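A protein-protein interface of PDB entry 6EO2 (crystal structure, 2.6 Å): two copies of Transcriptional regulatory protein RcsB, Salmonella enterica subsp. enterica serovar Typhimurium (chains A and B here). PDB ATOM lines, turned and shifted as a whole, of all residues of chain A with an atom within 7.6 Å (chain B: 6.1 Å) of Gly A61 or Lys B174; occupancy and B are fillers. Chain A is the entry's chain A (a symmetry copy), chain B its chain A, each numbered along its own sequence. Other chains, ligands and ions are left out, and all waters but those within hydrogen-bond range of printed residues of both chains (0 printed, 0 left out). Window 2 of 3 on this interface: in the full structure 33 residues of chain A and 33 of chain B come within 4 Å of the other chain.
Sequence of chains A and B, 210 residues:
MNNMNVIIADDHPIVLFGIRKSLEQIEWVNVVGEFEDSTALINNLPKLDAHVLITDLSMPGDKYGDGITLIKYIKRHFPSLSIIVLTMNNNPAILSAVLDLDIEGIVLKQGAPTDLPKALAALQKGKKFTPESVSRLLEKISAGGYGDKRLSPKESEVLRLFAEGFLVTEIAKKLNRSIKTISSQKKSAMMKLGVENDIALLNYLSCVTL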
ATOM      1  N   ASP A  11     -13.535  34.140   9.776  1.00  0.00           N
ATOM      2  CA  ASP A  11     -14.793  34.789   9.440  1.00  0.00           C
ATOM      3  C   ASP A  11     -15.052  36.031  10.307  1.00  0.00           C
ATOM      4  O   ASP A  11     -15.488  37.055   9.799  1.00  0.00           O
ATOM      5  CB  ASP A  11     -15.942  33.777   9.605  1.00  0.00           C
ATOM      6  CG  ASP A  11     -16.998  33.899   8.523  1.00  0.00           C
ATOM      7  OD1 ASP A  11     -16.681  34.326   7.385  1.00  0.00           O
ATOM      8  OD2 ASP A  11     -18.155  33.534   8.812  1.00  0.00           O
ATOM      9  N   ASP A  37     -12.509  36.057   4.215  1.00  0.00           N
ATOM     10  CA  ASP A  37     -13.115  35.044   3.354  1.00  0.00           C
ATOM     11  C   ASP A  37     -12.038  34.305   2.567  1.00  0.00           C
ATOM     12  O   ASP A  37     -10.949  34.840   2.308  1.00  0.00           O
ATOM     13  CB  ASP A  37     -14.137  35.662   2.401  1.00  0.00           C
ATOM     14  CG  ASP A  37     -13.499  36.581   1.399  1.00  0.00           C
ATOM     15  OD1 ASP A  37     -12.845  37.560   1.825  1.00  0.00           O
ATOM     16  OD2 ASP A  37     -13.638  36.315   0.188  1.00  0.00           O
ATOM     17  N   SER A  38     -12.363  33.075   2.185  1.00  0.00           N
ATOM     18  CA  SER A  38     -11.397  32.187   1.563  1.00  0.00           C
ATOM     19  C   SER A  38     -10.961  32.697   0.193  1.00  0.00           C
ATOM     20  O   SER A  38      -9.829  32.510  -0.202  1.00  0.00           O
ATOM     21  CB  SER A  38     -11.974  30.772   1.454  1.00  0.00           C
ATOM     22  OG  SER A  38     -13.142  30.764   0.661  1.00  0.00           O
ATOM     23  N   THR A  39     -11.858  33.357  -0.522  1.00  0.00           N
ATOM     24  CA  THR A  39     -11.540  33.884  -1.842  1.00  0.00           C
ATOM     25  C   THR A  39     -10.442  34.948  -1.838  1.00  0.00           C
ATOM     26  O   THR A  39      -9.579  34.957  -2.712  1.00  0.00           O
ATOM     27  CB  THR A  39     -12.798  34.456  -2.515  1.00  0.00           C
ATOM     28  OG1 THR A  39     -13.757  33.402  -2.712  1.00  0.00           O
ATOM     29  CG2 THR A  39     -12.449  35.093  -3.860  1.00  0.00           C
ATOM     30  N   SER A  58     -14.227  26.364   9.455  1.00  0.00           N
ATOM     31  CA  SER A  58     -15.523  26.659   8.881  1.00  0.00           C
ATOM     32  C   SER A  58     -15.603  28.036   8.209  1.00  0.00           C
ATOM     33  O   SER A  58     -16.561  28.771   8.428  1.00  0.00           O
ATOM     34  CB  SER A  58     -16.554  26.597  10.004  1.00  0.00           C
ATOM     35  OG  SER A  58     -16.411  27.714  10.866  1.00  0.00           O
ATOM     36  N   MET A  59     -14.623  28.392   7.390  1.00  0.00           N
ATOM     37  CA  MET A  59     -14.670  29.683   6.706  1.00  0.00           C
ATOM     38  C   MET A  59     -15.460  29.584   5.401  1.00  0.00           C
ATOM     39  O   MET A  59     -15.312  28.603   4.652  1.00  0.00           O
ATOM     40  CB  MET A  59     -13.263  30.191   6.420  1.00  0.00           C
ATOM     41  CG  MET A  59     -13.189  31.702   6.346  1.00  0.00           C
ATOM     42  SD  MET A  59     -11.502  32.295   6.376  1.00  0.00           S
ATOM     43  CE  MET A  59     -10.920  31.458   4.905  1.00  0.00           C
ATOM     44  N   PRO A  60     -16.285  30.610   5.108  1.00  0.00           N
ATOM     45  CA  PRO A  60     -17.123  30.578   3.914  1.00  0.00           C
ATOM     46  C   PRO A  60     -16.335  30.840   2.641  1.00  0.00           C
ATOM     47  O   PRO A  60     -15.681  31.886   2.513  1.00  0.00           O
ATOM     48  CB  PRO A  60     -18.105  31.726   4.153  1.00  0.00           C
ATOM     49  CG  PRO A  60     -17.324  32.714   4.946  1.00  0.00           C
ATOM     50  CD  PRO A  60     -16.448  31.883   5.844  1.00  0.00           C
ATOM     51  N   GLY A  61     -16.401  29.881   1.720  1.00  0.00           N
ATOM     52  CA  GLY A  61     -15.834  30.037   0.390  1.00  0.00           C
ATOM     53  C   GLY A  61     -16.880  29.936  -0.698  1.00  0.00           C
ATOM     54  O   GLY A  61     -17.514  28.890  -0.858  1.00  0.00           O
ATOM     55  N   ASP A  62     -17.051  31.016  -1.454  1.00  0.00           N
ATOM     56  CA  ASP A  62     -17.941  30.999  -2.624  1.00  0.00           C
ATOM     57  C   ASP A  62     -17.292  30.410  -3.889  1.00  0.00           C
ATOM     58  O   ASP A  62     -17.986  30.158  -4.866  1.00  0.00           O
ATOM     59  CB  ASP A  62     -18.486  32.409  -2.925  1.00  0.00           C
ATOM     60  CG  ASP A  62     -17.403  33.388  -3.400  1.00  0.00           C
ATOM     61  OD1 ASP A  62     -16.455  33.666  -2.629  1.00  0.00           O
ATOM     62  OD2 ASP A  62     -17.516  33.893  -4.543  1.00  0.00           O
ATOM     63  N   LYS A  63     -15.975  30.194  -3.866  1.00  0.00           N
ATOM     64  CA  LYS A  63     -15.229  29.717  -5.036  1.00  0.00           C
ATOM     65  C   LYS A  63     -14.449  28.431  -4.804  1.00  0.00           C
ATOM     66  O   LYS A  63     -14.562  27.496  -5.585  1.00  0.00           O
ATOM     67  CB  LYS A  63     -14.228  30.783  -5.485  1.00  0.00           C
ATOM     68  CG  LYS A  63     -14.674  31.605  -6.675  1.00  0.00           C
ATOM     69  CD  LYS A  63     -13.671  32.702  -6.970  1.00  0.00           C
ATOM     70  CE  LYS A  63     -14.316  33.839  -7.731  1.00  0.00           C
ATOM     71  NZ  LYS A  63     -15.317  34.586  -6.910  1.00  0.00           N
ATOM     72  N   TYR A  64     -13.643  28.407  -3.743  1.00  0.00           N
ATOM     73  CA  TYR A  64     -12.608  27.388  -3.564  1.00  0.00           C
ATOM     74  C   TYR A  64     -12.951  26.267  -2.563  1.00  0.00           C
ATOM     75  O   TYR A  64     -12.073  25.503  -2.145  1.00  0.00           O
ATOM     76  CB  TYR A  64     -11.304  28.076  -3.157  1.00  0.00           C
ATOM     77  CG  TYR A  64     -10.848  29.130  -4.141  1.00  0.00           C
ATOM     78  CD1 TYR A  64     -10.467  28.782  -5.435  1.00  0.00           C
ATOM     79  CD2 TYR A  64     -10.779  30.471  -3.779  1.00  0.00           C
ATOM     80  CE1 TYR A  64     -10.050  29.742  -6.344  1.00  0.00           C
ATOM     81  CE2 TYR A  64     -10.355  31.438  -4.685  1.00  0.00           C
ATOM     82  CZ  TYR A  64      -9.992  31.063  -5.965  1.00  0.00           C
ATOM     83  OH  TYR A  64      -9.570  32.015  -6.858  1.00  0.00           O
ATOM     84  N   GLY A  65     -14.225  26.158  -2.193  1.00  0.00           N
ATOM     85  CA  GLY A  65     -14.685  25.082  -1.320  1.00  0.00           C
ATOM     86  C   GLY A  65     -14.945  25.554   0.087  1.00  0.00           C
ATOM     87  O   GLY A  65     -14.696  26.706   0.425  1.00  0.00           O
ATOM     88  N   ASP A  66     -15.453  24.647   0.906  1.00  0.00           N
ATOM     89  CA  ASP A  66     -15.771  24.931   2.300  1.00  0.00           C
ATOM     90  C   ASP A  66     -15.096  23.926   3.223  1.00  0.00           C
ATOM     91  O   ASP A  66     -14.849  22.770   2.842  1.00  0.00           O
ATOM     92  CB  ASP A  66     -17.275  24.838   2.524  1.00  0.00           C
ATOM     93  CG  ASP A  66     -18.052  25.822   1.689  1.00  0.00           C
ATOM     94  OD1 ASP A  66     -17.990  27.044   1.978  1.00  0.00           O
ATOM     95  OD2 ASP A  66     -18.738  25.363   0.757  1.00  0.00           O
ATOM     96  N   GLY A  67     -14.804  24.367   4.441  1.00  0.00           N
ATOM     97  CA  GLY A  67     -14.404  23.455   5.494  1.00  0.00           C
ATOM     98  C   GLY A  67     -13.189  22.648   5.129  1.00  0.00           C
ATOM     99  O   GLY A  67     -12.219  23.186   4.632  1.00  0.00           O
ATOM    100  N   LEU A  70     -11.736  22.966   1.728  1.00  0.00           N
ATOM    101  CA  LEU A  70     -10.958  24.185   1.528  1.00  0.00           C
ATOM    102  C   LEU A  70      -9.528  24.004   2.032  1.00  0.00           C
ATOM    103  O   LEU A  70      -8.594  24.553   1.453  1.00  0.00           O
ATOM    104  CB  LEU A  70     -11.610  25.375   2.229  1.00  0.00           C
ATOM    105  CG  LEU A  70     -10.829  26.696   2.169  1.00  0.00           C
ATOM    106  CD1 LEU A  70     -10.669  27.180   0.739  1.00  0.00           C
ATOM    107  CD2 LEU A  70     -11.518  27.751   3.009  1.00  0.00           C
ATOM    108  N   GLU B 157     -27.612  19.731   1.074  1.00  0.00           N
ATOM    109  CA  GLU B 157     -26.688  20.826   1.290  1.00  0.00           C
ATOM    110  C   GLU B 157     -26.297  20.932   2.758  1.00  0.00           C
ATOM    111  O   GLU B 157     -25.119  21.035   3.089  1.00  0.00           O
ATOM    112  CB  GLU B 157     -27.335  22.125   0.820  1.00  0.00           C
ATOM    113  CG  GLU B 157     -26.455  23.357   0.926  1.00  0.00           C
ATOM    114  CD  GLU B 157     -25.131  23.228   0.189  1.00  0.00           C
ATOM    115  OE1 GLU B 157     -24.998  22.361  -0.711  1.00  0.00           O
ATOM    116  OE2 GLU B 157     -24.206  24.005   0.517  1.00  0.00           O
ATOM    117  N   ARG B 160     -23.984  18.151   3.576  1.00  0.00           N
ATOM    118  CA  ARG B 160     -22.702  18.429   2.928  1.00  0.00           C
ATOM    119  C   ARG B 160     -21.822  19.316   3.808  1.00  0.00           C
ATOM    120  O   ARG B 160     -20.639  19.038   3.990  1.00  0.00           O
ATOM    121  CB  ARG B 160     -22.921  19.132   1.587  1.00  0.00           C
ATOM    122  CG  ARG B 160     -21.828  18.874   0.566  1.00  0.00           C
ATOM    123  CD  ARG B 160     -21.748  19.995  -0.451  1.00  0.00           C
ATOM    124  NE  ARG B 160     -20.755  20.986  -0.037  1.00  0.00           N
ATOM    125  CZ  ARG B 160     -20.949  22.304   0.039  1.00  0.00           C
ATOM    126  NH1 ARG B 160     -19.958  23.089   0.434  1.00  0.00           N
ATOM    127  NH2 ARG B 160     -22.111  22.847  -0.281  1.00  0.00           N
ATOM    128  N   LEU B 161     -22.413  20.376   4.354  1.00  0.00           N
ATOM    129  CA  LEU B 161     -21.676  21.325   5.178  1.00  0.00           C
ATOM    130  C   LEU B 161     -21.339  20.739   6.531  1.00  0.00           C
ATOM    131  O   LEU B 161     -20.244  20.960   7.046  1.00  0.00           O
ATOM    132  CB  LEU B 161     -22.465  22.623   5.355  1.00  0.00           C
ATOM    133  CG  LEU B 161     -22.617  23.435   4.069  1.00  0.00           C
ATOM    134  CD1 LEU B 161     -23.567  24.608   4.257  1.00  0.00           C
ATOM    135  CD2 LEU B 161     -21.254  23.905   3.584  1.00  0.00           C
ATOM    136  N   PHE B 166     -18.729  22.198   9.399  1.00  0.00           N
ATOM    137  CA  PHE B 166     -19.523  23.330   9.880  1.00  0.00           C
ATOM    138  C   PHE B 166     -20.467  22.876  10.998  1.00  0.00           C
ATOM    139  O   PHE B 166     -21.116  21.836  10.882  1.00  0.00           O
ATOM    140  CB  PHE B 166     -20.376  23.922   8.752  1.00  0.00           C
ATOM    141  CG  PHE B 166     -19.605  24.751   7.755  1.00  0.00           C
ATOM    142  CD1 PHE B 166     -18.598  24.191   6.987  1.00  0.00           C
ATOM    143  CD2 PHE B 166     -19.922  26.088   7.554  1.00  0.00           C
ATOM    144  CE1 PHE B 166     -17.909  24.948   6.058  1.00  0.00           C
ATOM    145  CE2 PHE B 166     -19.235  26.852   6.622  1.00  0.00           C
ATOM    146  CZ  PHE B 166     -18.226  26.283   5.873  1.00  0.00           C
ATOM    147  N   THR B 169     -24.900  26.364  13.543  1.00  0.00           N
ATOM    148  CA  THR B 169     -25.025  27.823  13.553  1.00  0.00           C
ATOM    149  C   THR B 169     -24.269  28.432  12.365  1.00  0.00           C
ATOM    150  O   THR B 169     -24.745  29.389  11.744  1.00  0.00           O
ATOM    151  CB  THR B 169     -24.565  28.447  14.892  1.00  0.00           C
ATOM    152  OG1 THR B 169     -23.172  28.198  15.105  1.00  0.00           O
ATOM    153  CG2 THR B 169     -25.375  27.867  16.065  1.00  0.00           C
ATOM    154  N   GLU B 170     -23.118  27.846  12.037  1.00  0.00           N
ATOM    155  CA  GLU B 170     -22.332  28.252  10.872  1.00  0.00           C
ATOM    156  C   GLU B 170     -23.055  27.955   9.553  1.00  0.00           C
ATOM    157  O   GLU B 170     -22.923  28.705   8.581  1.00  0.00           O
ATOM    158  CB  GLU B 170     -20.966  27.560  10.886  1.00  0.00           C
ATOM    159  CG  GLU B 170     -20.067  27.981  12.046  1.00  0.00           C
ATOM    160  CD  GLU B 170     -18.979  26.970  12.394  1.00  0.00           C
ATOM    161  OE1 GLU B 170     -18.943  25.870  11.810  1.00  0.00           O
ATOM    162  OE2 GLU B 170     -18.151  27.268  13.279  1.00  0.00           O
ATOM    163  N   ILE B 171     -23.819  26.867   9.520  1.00  0.00           N
ATOM    164  CA  ILE B 171     -24.574  26.506   8.329  1.00  0.00           C
ATOM    165  C   ILE B 171     -25.707  27.495   8.096  1.00  0.00           C
ATOM    166  O   ILE B 171     -25.980  27.864   6.951  1.00  0.00           O
ATOM    167  CB  ILE B 171     -25.142  25.070   8.421  1.00  0.00           C
ATOM    168  CG1 ILE B 171     -23.992  24.052   8.481  1.00  0.00           C
ATOM    169  CG2 ILE B 171     -26.059  24.773   7.233  1.00  0.00           C
ATOM    170  CD1 ILE B 171     -24.427  22.611   8.643  1.00  0.00           C
ATOM    171  N   ALA B 172     -26.375  27.903   9.175  1.00  0.00           N
ATOM    172  CA  ALA B 172     -27.459  28.897   9.098  1.00  0.00           C
ATOM    173  C   ALA B 172     -26.978  30.201   8.451  1.00  0.00           C
ATOM    174  O   ALA B 172     -27.652  30.778   7.603  1.00  0.00           O
ATOM    175  CB  ALA B 172     -28.004  29.176  10.488  1.00  0.00           C
ATOM    176  N   LYS B 173     -25.797  30.645   8.862  1.00  0.00           N
ATOM    177  CA  LYS B 173     -25.182  31.839   8.311  1.00  0.00           C
ATOM    178  C   LYS B 173     -24.832  31.584   6.858  1.00  0.00           C
ATOM    179  O   LYS B 173     -25.341  32.256   5.967  1.00  0.00           O
ATOM    180  CB  LYS B 173     -23.923  32.202   9.103  1.00  0.00           C
ATOM    181  CG  LYS B 173     -23.825  33.674   9.461  1.00  0.00           C
ATOM    182  CD  LYS B 173     -23.048  33.881  10.755  1.00  0.00           C
ATOM    183  CE  LYS B 173     -23.882  33.519  11.981  1.00  0.00           C
ATOM    184  NZ  LYS B 173     -23.060  33.461  13.224  1.00  0.00           N
ATOM    185  N   LYS B 174     -23.992  30.583   6.623  1.00  0.00           N
ATOM    186  CA  LYS B 174     -23.588  30.218   5.272  1.00  0.00           C
ATOM    187  C   LYS B 174     -24.776  30.160   4.307  1.00  0.00           C
ATOM    188  O   LYS B 174     -24.697  30.696   3.203  1.00  0.00           O
ATOM    189  CB  LYS B 174     -22.851  28.876   5.301  1.00  0.00           C
ATOM    190  CG  LYS B 174     -22.518  28.277   3.938  1.00  0.00           C
ATOM    191  CD  LYS B 174     -21.359  28.979   3.256  1.00  0.00           C
ATOM    192  CE  LYS B 174     -21.081  28.373   1.890  1.00  0.00           C
ATOM    193  NZ  LYS B 174     -19.752  28.802   1.375  1.00  0.00           N
ATOM    194  N   LEU B 175     -25.871  29.519   4.720  1.00  0.00           N
ATOM    195  CA  LEU B 175     -27.010  29.285   3.828  1.00  0.00           C
ATOM    196  C   LEU B 175     -28.099  30.343   3.930  1.00  0.00           C
ATOM    197  O   LEU B 175     -29.036  30.343   3.125  1.00  0.00           O
ATOM    198  CB  LEU B 175     -27.628  27.906   4.086  1.00  0.00           C
ATOM    199  CG  LEU B 175     -26.781  26.695   3.690  1.00  0.00           C
ATOM    200  CD1 LEU B 175     -27.548  25.405   3.931  1.00  0.00           C
ATOM    201  CD2 LEU B 175     -26.336  26.790   2.240  1.00  0.00           C
ATOM    202  N   ASN B 176     -27.988  31.230   4.916  1.00  0.00           N
ATOM    203  CA  ASN B 176     -28.953  32.310   5.103  1.00  0.00           C
ATOM    204  C   ASN B 176     -30.374  31.787   5.361  1.00  0.00           C
ATOM    205  O   ASN B 176     -31.317  32.109   4.635  1.00  0.00           O
ATOM    206  CB  ASN B 176     -28.921  33.266   3.903  1.00  0.00           C
ATOM    207  CG  ASN B 176     -29.468  34.636   4.238  1.00  0.00           C
ATOM    208  OD1 ASN B 176     -30.566  34.994   3.813  1.00  0.00           O
ATOM    209  ND2 ASN B 176     -28.709  35.407   5.017  1.00  0.00           N
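OE2 of Glu B157 lies within salt-bridge range of NH2 of Arg B160 (2.5 Å).
N of Phe B166 sits at hydrogen-bond distance from O of Leu B161 (3.1 Å).
N of Gly A61 lies within hydrogen-bond range of OD1 of Asp A66.
Printed residues of chain A that touch a printed residue of chain B: Ser A58, Met A59, Gly A61, Asp A66 and Gly A67.
Of the 12 printed residues of chain B, 4 touch a printed residue of chain A.
Among the printed residues, 8 pairs touch across the chains.
Of the printed residues of chain B, Ser A58 touches Phe B166 and Glu B170.
Of the printed residues of chain B, Met A59 touches Phe B166.
Gly A61 touches just one residue of chain B: Lys B174.
Of the printed residues of chain A, Arg B160 touches Asp A66 (2.6 Å).
Printed residues of chain A within 4 Å of Glu B170: Ser A58.
Lys B174 touches just these residues of chain A: Gly A61 and Asp A66.
The nearest residue of chain B that does not touch Gly A61 is Phe B166 (5.8 Å).
The nearest residue of chain A that does not touch Lys B174 is Pro A60 (4.1 Å).
No position is printed for both chains.
Of the 8 pairs that touch across the chains among the printed residues, none has its exchanged pair printed and touching as well.
The guanidinium group (NH1) of Arg B160 lies within salt-bridge range of the side-chain carboxylate (OD2) of Asp A66.
OE2 of Glu B170 sits at hydrogen-bond distance from OG of Ser A58 (3.0 Å).
NZ of Lys B174 sits at hydrogen-bond distance from O of Gly A61 (3.2 Å).
The side-chain amino group (NZ) of Lys B174 lies within salt-bridge range of the side-chain carboxylate (OD1) of Asp A66 (2.6 Å).
O of Ser A58 touches CE2 of Phe B166 (3.8 Å).
Phe B166 touches Met A59 (CZ to O, 3.9 Å).
CE1 of Phe B166 touches CB of Asp A66, at 3.6 Å.
Gly A67 touches Phe B166 (N to CE1, 3.5 Å).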
